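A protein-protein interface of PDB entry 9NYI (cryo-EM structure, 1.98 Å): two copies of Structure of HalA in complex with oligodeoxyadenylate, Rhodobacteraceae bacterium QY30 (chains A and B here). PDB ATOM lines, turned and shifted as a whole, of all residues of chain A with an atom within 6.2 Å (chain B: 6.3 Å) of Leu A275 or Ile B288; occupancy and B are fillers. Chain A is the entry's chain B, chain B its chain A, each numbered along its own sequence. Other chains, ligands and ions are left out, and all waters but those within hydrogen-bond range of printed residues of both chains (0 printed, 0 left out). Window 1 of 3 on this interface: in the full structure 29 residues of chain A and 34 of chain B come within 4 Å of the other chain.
NH2 of Arg B365 lies within hydrogen-bond range of OD1 of Asn A230 (3.3 Å). The guanidinium group of Arg A233 sits close to the guanidinium group of Arg B365 (3.0 Å).
NH1 of Arg B365 is in hydrogen-bond range of O of Ser B286. N of Arg B290 lies close to OG of Ser B287 (3.3 Å). O of Asn B282 is in hydrogen-bond range of N of Ser B287 (3.5 Å). O of Thr A226 lies close to OD1 of Asn A230 (3.2 Å).
O of Ser B286 touches NH1 of Arg A233, 3.5 Å away. Arg A233 touches Ser B287 (NH1 to CB, 3.7 Å). Leu A275 touches Ile B288. CD1 of Leu A275 touches NH2 of Arg B365, at 3.3 Å. Met A278 touches Ile B362 (CE to CG2, 3.9 Å). CE of Met A278 touches CD1 of Leu B366 (3.6 Å).
Printed residues of chain B within 4 Å of Leu A275: Ile B288 (3.99 Å) and Arg B365 (3.3 Å). Printed residues of chain A within 4 Å of Ile B288: Leu A275. Of the printed residues of chain A, Ile B362 touches Met A278. Printed residues of chain A within 4 Å of Ser B287: Arg A233. Trp A284 touches none of the printed residues of chain B. Ile A274 touches none of the printed residues of chain B. The nearest printed residue of chain A that does not touch Ile B288 is Ile A274 (4.7 Å).
Printed residues of chain B that touch a printed residue of chain A: Ser B286, Ser B287, Ile B288, Ile B362, Arg B365 and Leu B366. Hydrophobic or aromatic side chains of chain B that line the printed part of chain A: Ile B288, Ile B362 and Leu B366. Printed residues of chain A that touch a printed residue of chain B: Asn A230, Arg A233, Leu A275 and Met A278. Among the printed residues, 8 pairs touch across the chains.
No position is printed for both chains. Of the 8 pairs that touch across the chains among the printed residues, none has its exchanged pair printed and touching as well.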
ATOM      1  N   THR A 226      -3.189  13.515  11.393  1.00  0.00           N
ATOM      2  CA  THR A 226      -4.197  14.376  12.004  1.00  0.00           C
ATOM      3  C   THR A 226      -5.031  15.078  10.935  1.00  0.00           C
ATOM      4  O   THR A 226      -6.274  15.069  10.983  1.00  0.00           O
ATOM      5  CB  THR A 226      -3.525  15.401  12.918  1.00  0.00           C
ATOM      6  OG1 THR A 226      -2.795  14.720  13.944  1.00  0.00           O
ATOM      7  CG2 THR A 226      -4.572  16.291  13.565  1.00  0.00           C
ATOM      8  N   ASN A 230      -9.135  14.473  10.136  1.00  0.00           N
ATOM      9  CA  ASN A 230     -10.146  15.526  10.170  1.00  0.00           C
ATOM     10  C   ASN A 230     -10.793  15.733   8.800  1.00  0.00           C
ATOM     11  O   ASN A 230     -11.999  16.000   8.719  1.00  0.00           O
ATOM     12  CB  ASN A 230      -9.541  16.816  10.716  1.00  0.00           C
ATOM     13  CG  ASN A 230      -9.337  16.786  12.213  1.00  0.00           C
ATOM     14  OD1 ASN A 230      -8.211  16.882  12.701  1.00  0.00           O
ATOM     15  ND2 ASN A 230     -10.430  16.650  12.952  1.00  0.00           N
ATOM     16  N   ARG A 233     -13.355  13.036   8.521  1.00  0.00           N
ATOM     17  CA  ARG A 233     -14.550  13.403   9.280  1.00  0.00           C
ATOM     18  C   ARG A 233     -15.416  14.387   8.497  1.00  0.00           C
ATOM     19  O   ARG A 233     -16.639  14.217   8.399  1.00  0.00           O
ATOM     20  CB  ARG A 233     -14.151  13.989  10.633  1.00  0.00           C
ATOM     21  CG  ARG A 233     -13.799  12.945  11.677  1.00  0.00           C
ATOM     22  CD  ARG A 233     -13.240  13.590  12.932  1.00  0.00           C
ATOM     23  NE  ARG A 233     -12.194  12.776  13.538  1.00  0.00           N
ATOM     24  CZ  ARG A 233     -12.046  12.598  14.844  1.00  0.00           C
ATOM     25  NH1 ARG A 233     -12.857  13.175  15.716  1.00  0.00           N
ATOM     26  NH2 ARG A 233     -11.060  11.821  15.285  1.00  0.00           N
ATOM     27  N   VAL A 270     -14.402  22.603  13.251  1.00  0.00           N
ATOM     28  CA  VAL A 270     -13.910  23.209  14.482  1.00  0.00           C
ATOM     29  C   VAL A 270     -12.668  22.463  14.952  1.00  0.00           C
ATOM     30  O   VAL A 270     -11.673  23.070  15.372  1.00  0.00           O
ATOM     31  CB  VAL A 270     -15.013  23.228  15.556  1.00  0.00           C
ATOM     32  CG1 VAL A 270     -14.431  23.551  16.916  1.00  0.00           C
ATOM     33  CG2 VAL A 270     -16.078  24.252  15.193  1.00  0.00           C
ATOM     34  N   GLY A 271     -12.693  21.132  14.855  1.00  0.00           N
ATOM     35  CA  GLY A 271     -11.536  20.372  15.288  1.00  0.00           C
ATOM     36  C   GLY A 271     -10.377  20.546  14.325  1.00  0.00           C
ATOM     37  O   GLY A 271      -9.221  20.595  14.753  1.00  0.00           O
ATOM     38  N   MET A 272     -10.664  20.698  13.028  1.00  0.00           N
ATOM     39  CA  MET A 272      -9.619  21.096  12.090  1.00  0.00           C
ATOM     40  C   MET A 272      -8.944  22.372  12.562  1.00  0.00           C
ATOM     41  O   MET A 272      -7.714  22.444  12.665  1.00  0.00           O
ATOM     42  CB  MET A 272     -10.197  21.308  10.685  1.00  0.00           C
ATOM     43  CG  MET A 272      -9.119  21.442   9.613  1.00  0.00           C
ATOM     44  SD  MET A 272      -8.095  19.991   9.322  1.00  0.00           S
ATOM     45  CE  MET A 272      -9.153  19.067   8.215  1.00  0.00           C
ATOM     46  N   LEU A 273      -9.749  23.389  12.872  1.00  0.00           N
ATOM     47  CA  LEU A 273      -9.194  24.695  13.217  1.00  0.00           C
ATOM     48  C   LEU A 273      -8.332  24.618  14.473  1.00  0.00           C
ATOM     49  O   LEU A 273      -7.178  25.070  14.478  1.00  0.00           O
ATOM     50  CB  LEU A 273     -10.323  25.712  13.390  1.00  0.00           C
ATOM     51  CG  LEU A 273     -11.131  26.030  12.131  1.00  0.00           C
ATOM     52  CD1 LEU A 273     -12.539  26.479  12.491  1.00  0.00           C
ATOM     53  CD2 LEU A 273     -10.425  27.081  11.288  1.00  0.00           C
ATOM     54  N   ILE A 274      -8.875  24.041  15.549  1.00  0.00           N
ATOM     55  CA  ILE A 274      -8.125  23.983  16.804  1.00  0.00           C
ATOM     56  C   ILE A 274      -6.866  23.135  16.649  1.00  0.00           C
ATOM     57  O   ILE A 274      -5.787  23.515  17.120  1.00  0.00           O
ATOM     58  CB  ILE A 274      -9.012  23.486  17.962  1.00  0.00           C
ATOM     59  CG1 ILE A 274      -9.911  24.614  18.482  1.00  0.00           C
ATOM     60  CG2 ILE A 274      -8.156  22.962  19.100  1.00  0.00           C
ATOM     61  CD1 ILE A 274     -11.207  24.803  17.767  1.00  0.00           C
ATOM     62  N   LEU A 275      -6.977  21.973  15.998  1.00  0.00           N
ATOM     63  CA  LEU A 275      -5.808  21.110  15.862  1.00  0.00           C
ATOM     64  C   LEU A 275      -4.728  21.770  15.013  1.00  0.00           C
ATOM     65  O   LEU A 275      -3.538  21.669  15.329  1.00  0.00           O
ATOM     66  CB  LEU A 275      -6.222  19.759  15.282  1.00  0.00           C
ATOM     67  CG  LEU A 275      -6.919  18.885  16.328  1.00  0.00           C
ATOM     68  CD1 LEU A 275      -7.375  17.550  15.762  1.00  0.00           C
ATOM     69  CD2 LEU A 275      -6.041  18.683  17.557  1.00  0.00           C
ATOM     70  N   LEU A 276      -5.126  22.461  13.942  1.00  0.00           N
ATOM     71  CA  LEU A 276      -4.163  23.177  13.115  1.00  0.00           C
ATOM     72  C   LEU A 276      -3.458  24.262  13.916  1.00  0.00           C
ATOM     73  O   LEU A 276      -2.229  24.390  13.856  1.00  0.00           O
ATOM     74  CB  LEU A 276      -4.870  23.777  11.900  1.00  0.00           C
ATOM     75  CG  LEU A 276      -4.019  24.073  10.665  1.00  0.00           C
ATOM     76  CD1 LEU A 276      -3.329  22.811  10.176  1.00  0.00           C
ATOM     77  CD2 LEU A 276      -4.875  24.681   9.564  1.00  0.00           C
ATOM     78  N   VAL A 277      -4.217  25.041  14.691  1.00  0.00           N
ATOM     79  CA  VAL A 277      -3.605  26.112  15.478  1.00  0.00           C
ATOM     80  C   VAL A 277      -2.625  25.535  16.492  1.00  0.00           C
ATOM     81  O   VAL A 277      -1.485  25.999  16.622  1.00  0.00           O
ATOM     82  CB  VAL A 277      -4.689  26.967  16.160  1.00  0.00           C
ATOM     83  CG1 VAL A 277      -4.076  27.820  17.261  1.00  0.00           C
ATOM     84  CG2 VAL A 277      -5.400  27.836  15.136  1.00  0.00           C
ATOM     85  N   MET A 278      -3.047  24.495  17.216  1.00  0.00           N
ATOM     86  CA  MET A 278      -2.191  23.931  18.254  1.00  0.00           C
ATOM     87  C   MET A 278      -0.931  23.313  17.658  1.00  0.00           C
ATOM     88  O   MET A 278       0.175  23.516  18.176  1.00  0.00           O
ATOM     89  CB  MET A 278      -2.965  22.907  19.084  1.00  0.00           C
ATOM     90  CG  MET A 278      -4.175  23.492  19.801  1.00  0.00           C
ATOM     91  SD  MET A 278      -5.131  22.270  20.719  1.00  0.00           S
ATOM     92  CE  MET A 278      -3.955  21.792  21.980  1.00  0.00           C
ATOM     93  N   GLY A 279      -1.065  22.572  16.555  1.00  0.00           N
ATOM     94  CA  GLY A 279       0.102  21.907  16.003  1.00  0.00           C
ATOM     95  C   GLY A 279       1.048  22.870  15.312  1.00  0.00           C
ATOM     96  O   GLY A 279       2.266  22.669  15.329  1.00  0.00           O
ATOM     97  N   SER A 280       0.513  23.929  14.700  1.00  0.00           N
ATOM     98  CA  SER A 280       1.377  24.989  14.199  1.00  0.00           C
ATOM     99  C   SER A 280       2.097  25.693  15.341  1.00  0.00           C
ATOM    100  O   SER A 280       3.255  26.104  15.196  1.00  0.00           O
ATOM    101  CB  SER A 280       0.559  25.990  13.382  1.00  0.00           C
ATOM    102  OG  SER A 280      -0.149  25.340  12.341  1.00  0.00           O
ATOM    103  N   TRP A 284       3.543  20.365  16.270  1.00  0.00           N
ATOM    104  CA  TRP A 284       2.811  19.099  16.283  1.00  0.00           C
ATOM    105  C   TRP A 284       3.345  18.170  17.371  1.00  0.00           C
ATOM    106  O   TRP A 284       3.487  16.962  17.171  1.00  0.00           O
ATOM    107  CB  TRP A 284       2.835  18.433  14.906  1.00  0.00           C
ATOM    108  CG  TRP A 284       2.151  19.280  13.888  1.00  0.00           C
ATOM    109  CD1 TRP A 284       2.727  20.200  13.064  1.00  0.00           C
ATOM    110  CD2 TRP A 284       0.745  19.324  13.617  1.00  0.00           C
ATOM    111  NE1 TRP A 284       1.770  20.802  12.284  1.00  0.00           N
ATOM    112  CE2 TRP A 284       0.545  20.279  12.603  1.00  0.00           C
ATOM    113  CE3 TRP A 284      -0.361  18.638  14.126  1.00  0.00           C
ATOM    114  CZ2 TRP A 284      -0.717  20.567  12.088  1.00  0.00           C
ATOM    115  CZ3 TRP A 284      -1.613  18.925  13.613  1.00  0.00           C
ATOM    116  CH2 TRP A 284      -1.780  19.881  12.605  1.00  0.00           C
ATOM    117  N   ASN B 282     -17.105  12.970  25.309  1.00  0.00           N
ATOM    118  CA  ASN B 282     -15.918  13.321  24.536  1.00  0.00           C
ATOM    119  C   ASN B 282     -15.678  12.383  23.356  1.00  0.00           C
ATOM    120  O   ASN B 282     -14.567  12.356  22.815  1.00  0.00           O
ATOM    121  CB  ASN B 282     -14.678  13.387  25.434  1.00  0.00           C
ATOM    122  CG  ASN B 282     -14.297  12.040  26.031  1.00  0.00           C
ATOM    123  OD1 ASN B 282     -14.840  10.999  25.665  1.00  0.00           O
ATOM    124  ND2 ASN B 282     -13.351  12.061  26.961  1.00  0.00           N
ATOM    125  N   SER B 286     -12.026  10.893  21.212  1.00  0.00           N
ATOM    126  CA  SER B 286     -11.846  11.175  19.796  1.00  0.00           C
ATOM    127  C   SER B 286     -11.894  12.658  19.455  1.00  0.00           C
ATOM    128  O   SER B 286     -11.016  13.143  18.736  1.00  0.00           O
ATOM    129  CB  SER B 286     -12.903  10.436  18.969  1.00  0.00           C
ATOM    130  OG  SER B 286     -14.209  10.888  19.275  1.00  0.00           O
ATOM    131  N   SER B 287     -12.894  13.402  19.930  1.00  0.00           N
ATOM    132  CA  SER B 287     -13.212  14.695  19.333  1.00  0.00           C
ATOM    133  C   SER B 287     -13.148  15.779  20.404  1.00  0.00           C
ATOM    134  O   SER B 287     -13.975  15.804  21.323  1.00  0.00           O
ATOM    135  CB  SER B 287     -14.585  14.661  18.664  1.00  0.00           C
ATOM    136  OG  SER B 287     -15.581  15.189  19.516  1.00  0.00           O
ATOM    137  N   ILE B 288     -12.160  16.669  20.276  1.00  0.00           N
ATOM    138  CA  ILE B 288     -12.037  17.812  21.176  1.00  0.00           C
ATOM    139  C   ILE B 288     -13.231  18.743  21.026  1.00  0.00           C
ATOM    140  O   ILE B 288     -13.664  19.380  21.996  1.00  0.00           O
ATOM    141  CB  ILE B 288     -10.706  18.545  20.902  1.00  0.00           C
ATOM    142  CG1 ILE B 288      -9.518  17.647  21.249  1.00  0.00           C
ATOM    143  CG2 ILE B 288     -10.625  19.852  21.678  1.00  0.00           C
ATOM    144  CD1 ILE B 288      -8.180  18.256  20.899  1.00  0.00           C
ATOM    145  N   SER B 289     -13.788  18.829  19.815  1.00  0.00           N
ATOM    146  CA  SER B 289     -14.867  19.772  19.542  1.00  0.00           C
ATOM    147  C   SER B 289     -16.106  19.467  20.371  1.00  0.00           C
ATOM    148  O   SER B 289     -16.754  20.376  20.897  1.00  0.00           O
ATOM    149  CB  SER B 289     -15.221  19.738  18.058  1.00  0.00           C
ATOM    150  OG  SER B 289     -15.944  18.554  17.753  1.00  0.00           O
ATOM    151  N   ARG B 290     -16.444  18.182  20.519  1.00  0.00           N
ATOM    152  CA  ARG B 290     -17.611  17.820  21.320  1.00  0.00           C
ATOM    153  C   ARG B 290     -17.423  18.229  22.778  1.00  0.00           C
ATOM    154  O   ARG B 290     -18.360  18.720  23.417  1.00  0.00           O
ATOM    155  CB  ARG B 290     -17.868  16.317  21.225  1.00  0.00           C
ATOM    156  CG  ARG B 290     -18.876  15.807  22.232  1.00  0.00           C
ATOM    157  CD  ARG B 290     -19.183  14.329  22.059  1.00  0.00           C
ATOM    158  NE  ARG B 290     -19.136  13.925  20.661  1.00  0.00           N
ATOM    159  CZ  ARG B 290     -19.484  12.729  20.206  1.00  0.00           C
ATOM    160  NH1 ARG B 290     -20.030  11.822  20.998  1.00  0.00           N
ATOM    161  NH2 ARG B 290     -19.244  12.423  18.935  1.00  0.00           N
ATOM    162  N   ALA B 291     -16.223  18.017  23.323  1.00  0.00           N
ATOM    163  CA  ALA B 291     -15.951  18.433  24.695  1.00  0.00           C
ATOM    164  C   ALA B 291     -16.031  19.948  24.836  1.00  0.00           C
ATOM    165  O   ALA B 291     -16.591  20.461  25.813  1.00  0.00           O
ATOM    166  CB  ALA B 291     -14.583  17.916  25.137  1.00  0.00           C
ATOM    167  N   MET B 292     -15.489  20.680  23.859  1.00  0.00           N
ATOM    168  CA  MET B 292     -15.641  22.132  23.848  1.00  0.00           C
ATOM    169  C   MET B 292     -17.114  22.524  23.852  1.00  0.00           C
ATOM    170  O   MET B 292     -17.513  23.476  24.531  1.00  0.00           O
ATOM    171  CB  MET B 292     -14.938  22.722  22.625  1.00  0.00           C
ATOM    172  CG  MET B 292     -13.419  22.751  22.715  1.00  0.00           C
ATOM    173  SD  MET B 292     -12.794  22.792  24.403  1.00  0.00           S
ATOM    174  CE  MET B 292     -12.506  24.547  24.616  1.00  0.00           C
ATOM    175  N   LEU B 293     -17.938  21.782  23.112  1.00  0.00           N
ATOM    176  CA  LEU B 293     -19.343  22.144  22.978  1.00  0.00           C
ATOM    177  C   LEU B 293     -20.124  21.855  24.256  1.00  0.00           C
ATOM    178  O   LEU B 293     -20.978  22.657  24.649  1.00  0.00           O
ATOM    179  CB  LEU B 293     -19.956  21.419  21.780  1.00  0.00           C
ATOM    180  CG  LEU B 293     -21.365  21.830  21.339  1.00  0.00           C
ATOM    181  CD1 LEU B 293     -21.470  21.806  19.823  1.00  0.00           C
ATOM    182  CD2 LEU B 293     -22.420  20.923  21.957  1.00  0.00           C
ATOM    183  N   TRP B 354     -15.456  18.913  33.712  1.00  0.00           N
ATOM    184  CA  TRP B 354     -15.158  19.202  32.316  1.00  0.00           C
ATOM    185  C   TRP B 354     -13.660  19.125  32.042  1.00  0.00           C
ATOM    186  O   TRP B 354     -13.243  18.699  30.963  1.00  0.00           O
ATOM    187  CB  TRP B 354     -15.691  20.577  31.918  1.00  0.00           C
ATOM    188  CG  TRP B 354     -15.458  20.806  30.480  1.00  0.00           C
ATOM    189  CD1 TRP B 354     -16.243  20.394  29.447  1.00  0.00           C
ATOM    190  CD2 TRP B 354     -14.329  21.459  29.895  1.00  0.00           C
ATOM    191  NE1 TRP B 354     -15.684  20.768  28.252  1.00  0.00           N
ATOM    192  CE2 TRP B 354     -14.496  21.403  28.500  1.00  0.00           C
ATOM    193  CE3 TRP B 354     -13.194  22.089  30.417  1.00  0.00           C
ATOM    194  CZ2 TRP B 354     -13.583  21.973  27.619  1.00  0.00           C
ATOM    195  CZ3 TRP B 354     -12.273  22.625  29.541  1.00  0.00           C
ATOM    196  CH2 TRP B 354     -12.478  22.574  28.157  1.00  0.00           C
ATOM    197  N   ALA B 358     -12.015  16.814  29.229  1.00  0.00           N
ATOM    198  CA  ALA B 358     -11.412  17.455  28.069  1.00  0.00           C
ATOM    199  C   ALA B 358      -9.914  17.215  27.951  1.00  0.00           C
ATOM    200  O   ALA B 358      -9.402  17.097  26.834  1.00  0.00           O
ATOM    201  CB  ALA B 358     -11.688  18.961  28.103  1.00  0.00           C
ATOM    202  N   THR B 361      -8.776  14.222  25.782  1.00  0.00           N
ATOM    203  CA  THR B 361      -9.025  14.394  24.353  1.00  0.00           C
ATOM    204  C   THR B 361      -7.885  15.157  23.693  1.00  0.00           C
ATOM    205  O   THR B 361      -7.401  14.777  22.618  1.00  0.00           O
ATOM    206  CB  THR B 361     -10.349  15.123  24.120  1.00  0.00           C
ATOM    207  OG1 THR B 361     -10.152  16.539  24.247  1.00  0.00           O
ATOM    208  CG2 THR B 361     -11.417  14.664  25.089  1.00  0.00           C
ATOM    209  N   ILE B 362      -7.439  16.241  24.331  1.00  0.00           N
ATOM    210  CA  ILE B 362      -6.300  16.997  23.822  1.00  0.00           C
ATOM    211  C   ILE B 362      -5.050  16.128  23.820  1.00  0.00           C
ATOM    212  O   ILE B 362      -4.270  16.137  22.858  1.00  0.00           O
ATOM    213  CB  ILE B 362      -6.103  18.282  24.648  1.00  0.00           C
ATOM    214  CG1 ILE B 362      -7.195  19.300  24.317  1.00  0.00           C
ATOM    215  CG2 ILE B 362      -4.727  18.878  24.398  1.00  0.00           C
ATOM    216  CD1 ILE B 362      -7.351  20.383  25.360  1.00  0.00           C
ATOM    217  N   SER B 363      -4.845  15.359  24.893  1.00  0.00           N
ATOM    218  CA  SER B 363      -3.687  14.470  24.946  1.00  0.00           C
ATOM    219  C   SER B 363      -3.705  13.465  23.799  1.00  0.00           C
ATOM    220  O   SER B 363      -2.674  13.219  23.164  1.00  0.00           O
ATOM    221  CB  SER B 363      -3.641  13.748  26.293  1.00  0.00           C
ATOM    222  OG  SER B 363      -3.027  14.556  27.282  1.00  0.00           O
ATOM    223  N   ARG B 365      -5.304  13.737  20.849  1.00  0.00           N
ATOM    224  CA  ARG B 365      -5.170  14.368  19.541  1.00  0.00           C
ATOM    225  C   ARG B 365      -3.767  14.919  19.314  1.00  0.00           C
ATOM    226  O   ARG B 365      -3.352  15.091  18.163  1.00  0.00           O
ATOM    227  CB  ARG B 365      -6.210  15.474  19.375  1.00  0.00           C
ATOM    228  CG  ARG B 365      -7.646  14.974  19.348  1.00  0.00           C
ATOM    229  CD  ARG B 365      -7.793  13.741  18.470  1.00  0.00           C
ATOM    230  NE  ARG B 365      -7.709  14.057  17.050  1.00  0.00           N
ATOM    231  CZ  ARG B 365      -8.756  14.288  16.271  1.00  0.00           C
ATOM    232  NH1 ARG B 365      -9.990  14.268  16.749  1.00  0.00           N
ATOM    233  NH2 ARG B 365      -8.562  14.545  14.981  1.00  0.00           N
ATOM    234  N   LEU B 366      -3.024  15.199  20.385  1.00  0.00           N
ATOM    235  CA  LEU B 366      -1.670  15.722  20.242  1.00  0.00           C
ATOM    236  C   LEU B 366      -0.588  14.669  20.441  1.00  0.00           C
ATOM    237  O   LEU B 366       0.509  14.818  19.895  1.00  0.00           O
ATOM    238  CB  LEU B 366      -1.437  16.876  21.222  1.00  0.00           C
ATOM    239  CG  LEU B 366      -2.169  18.191  20.930  1.00  0.00           C
ATOM    240  CD1 LEU B 366      -1.333  19.372  21.389  1.00  0.00           C
ATOM    241  CD2 LEU B 366      -2.513  18.325  19.452  1.00  0.00           C
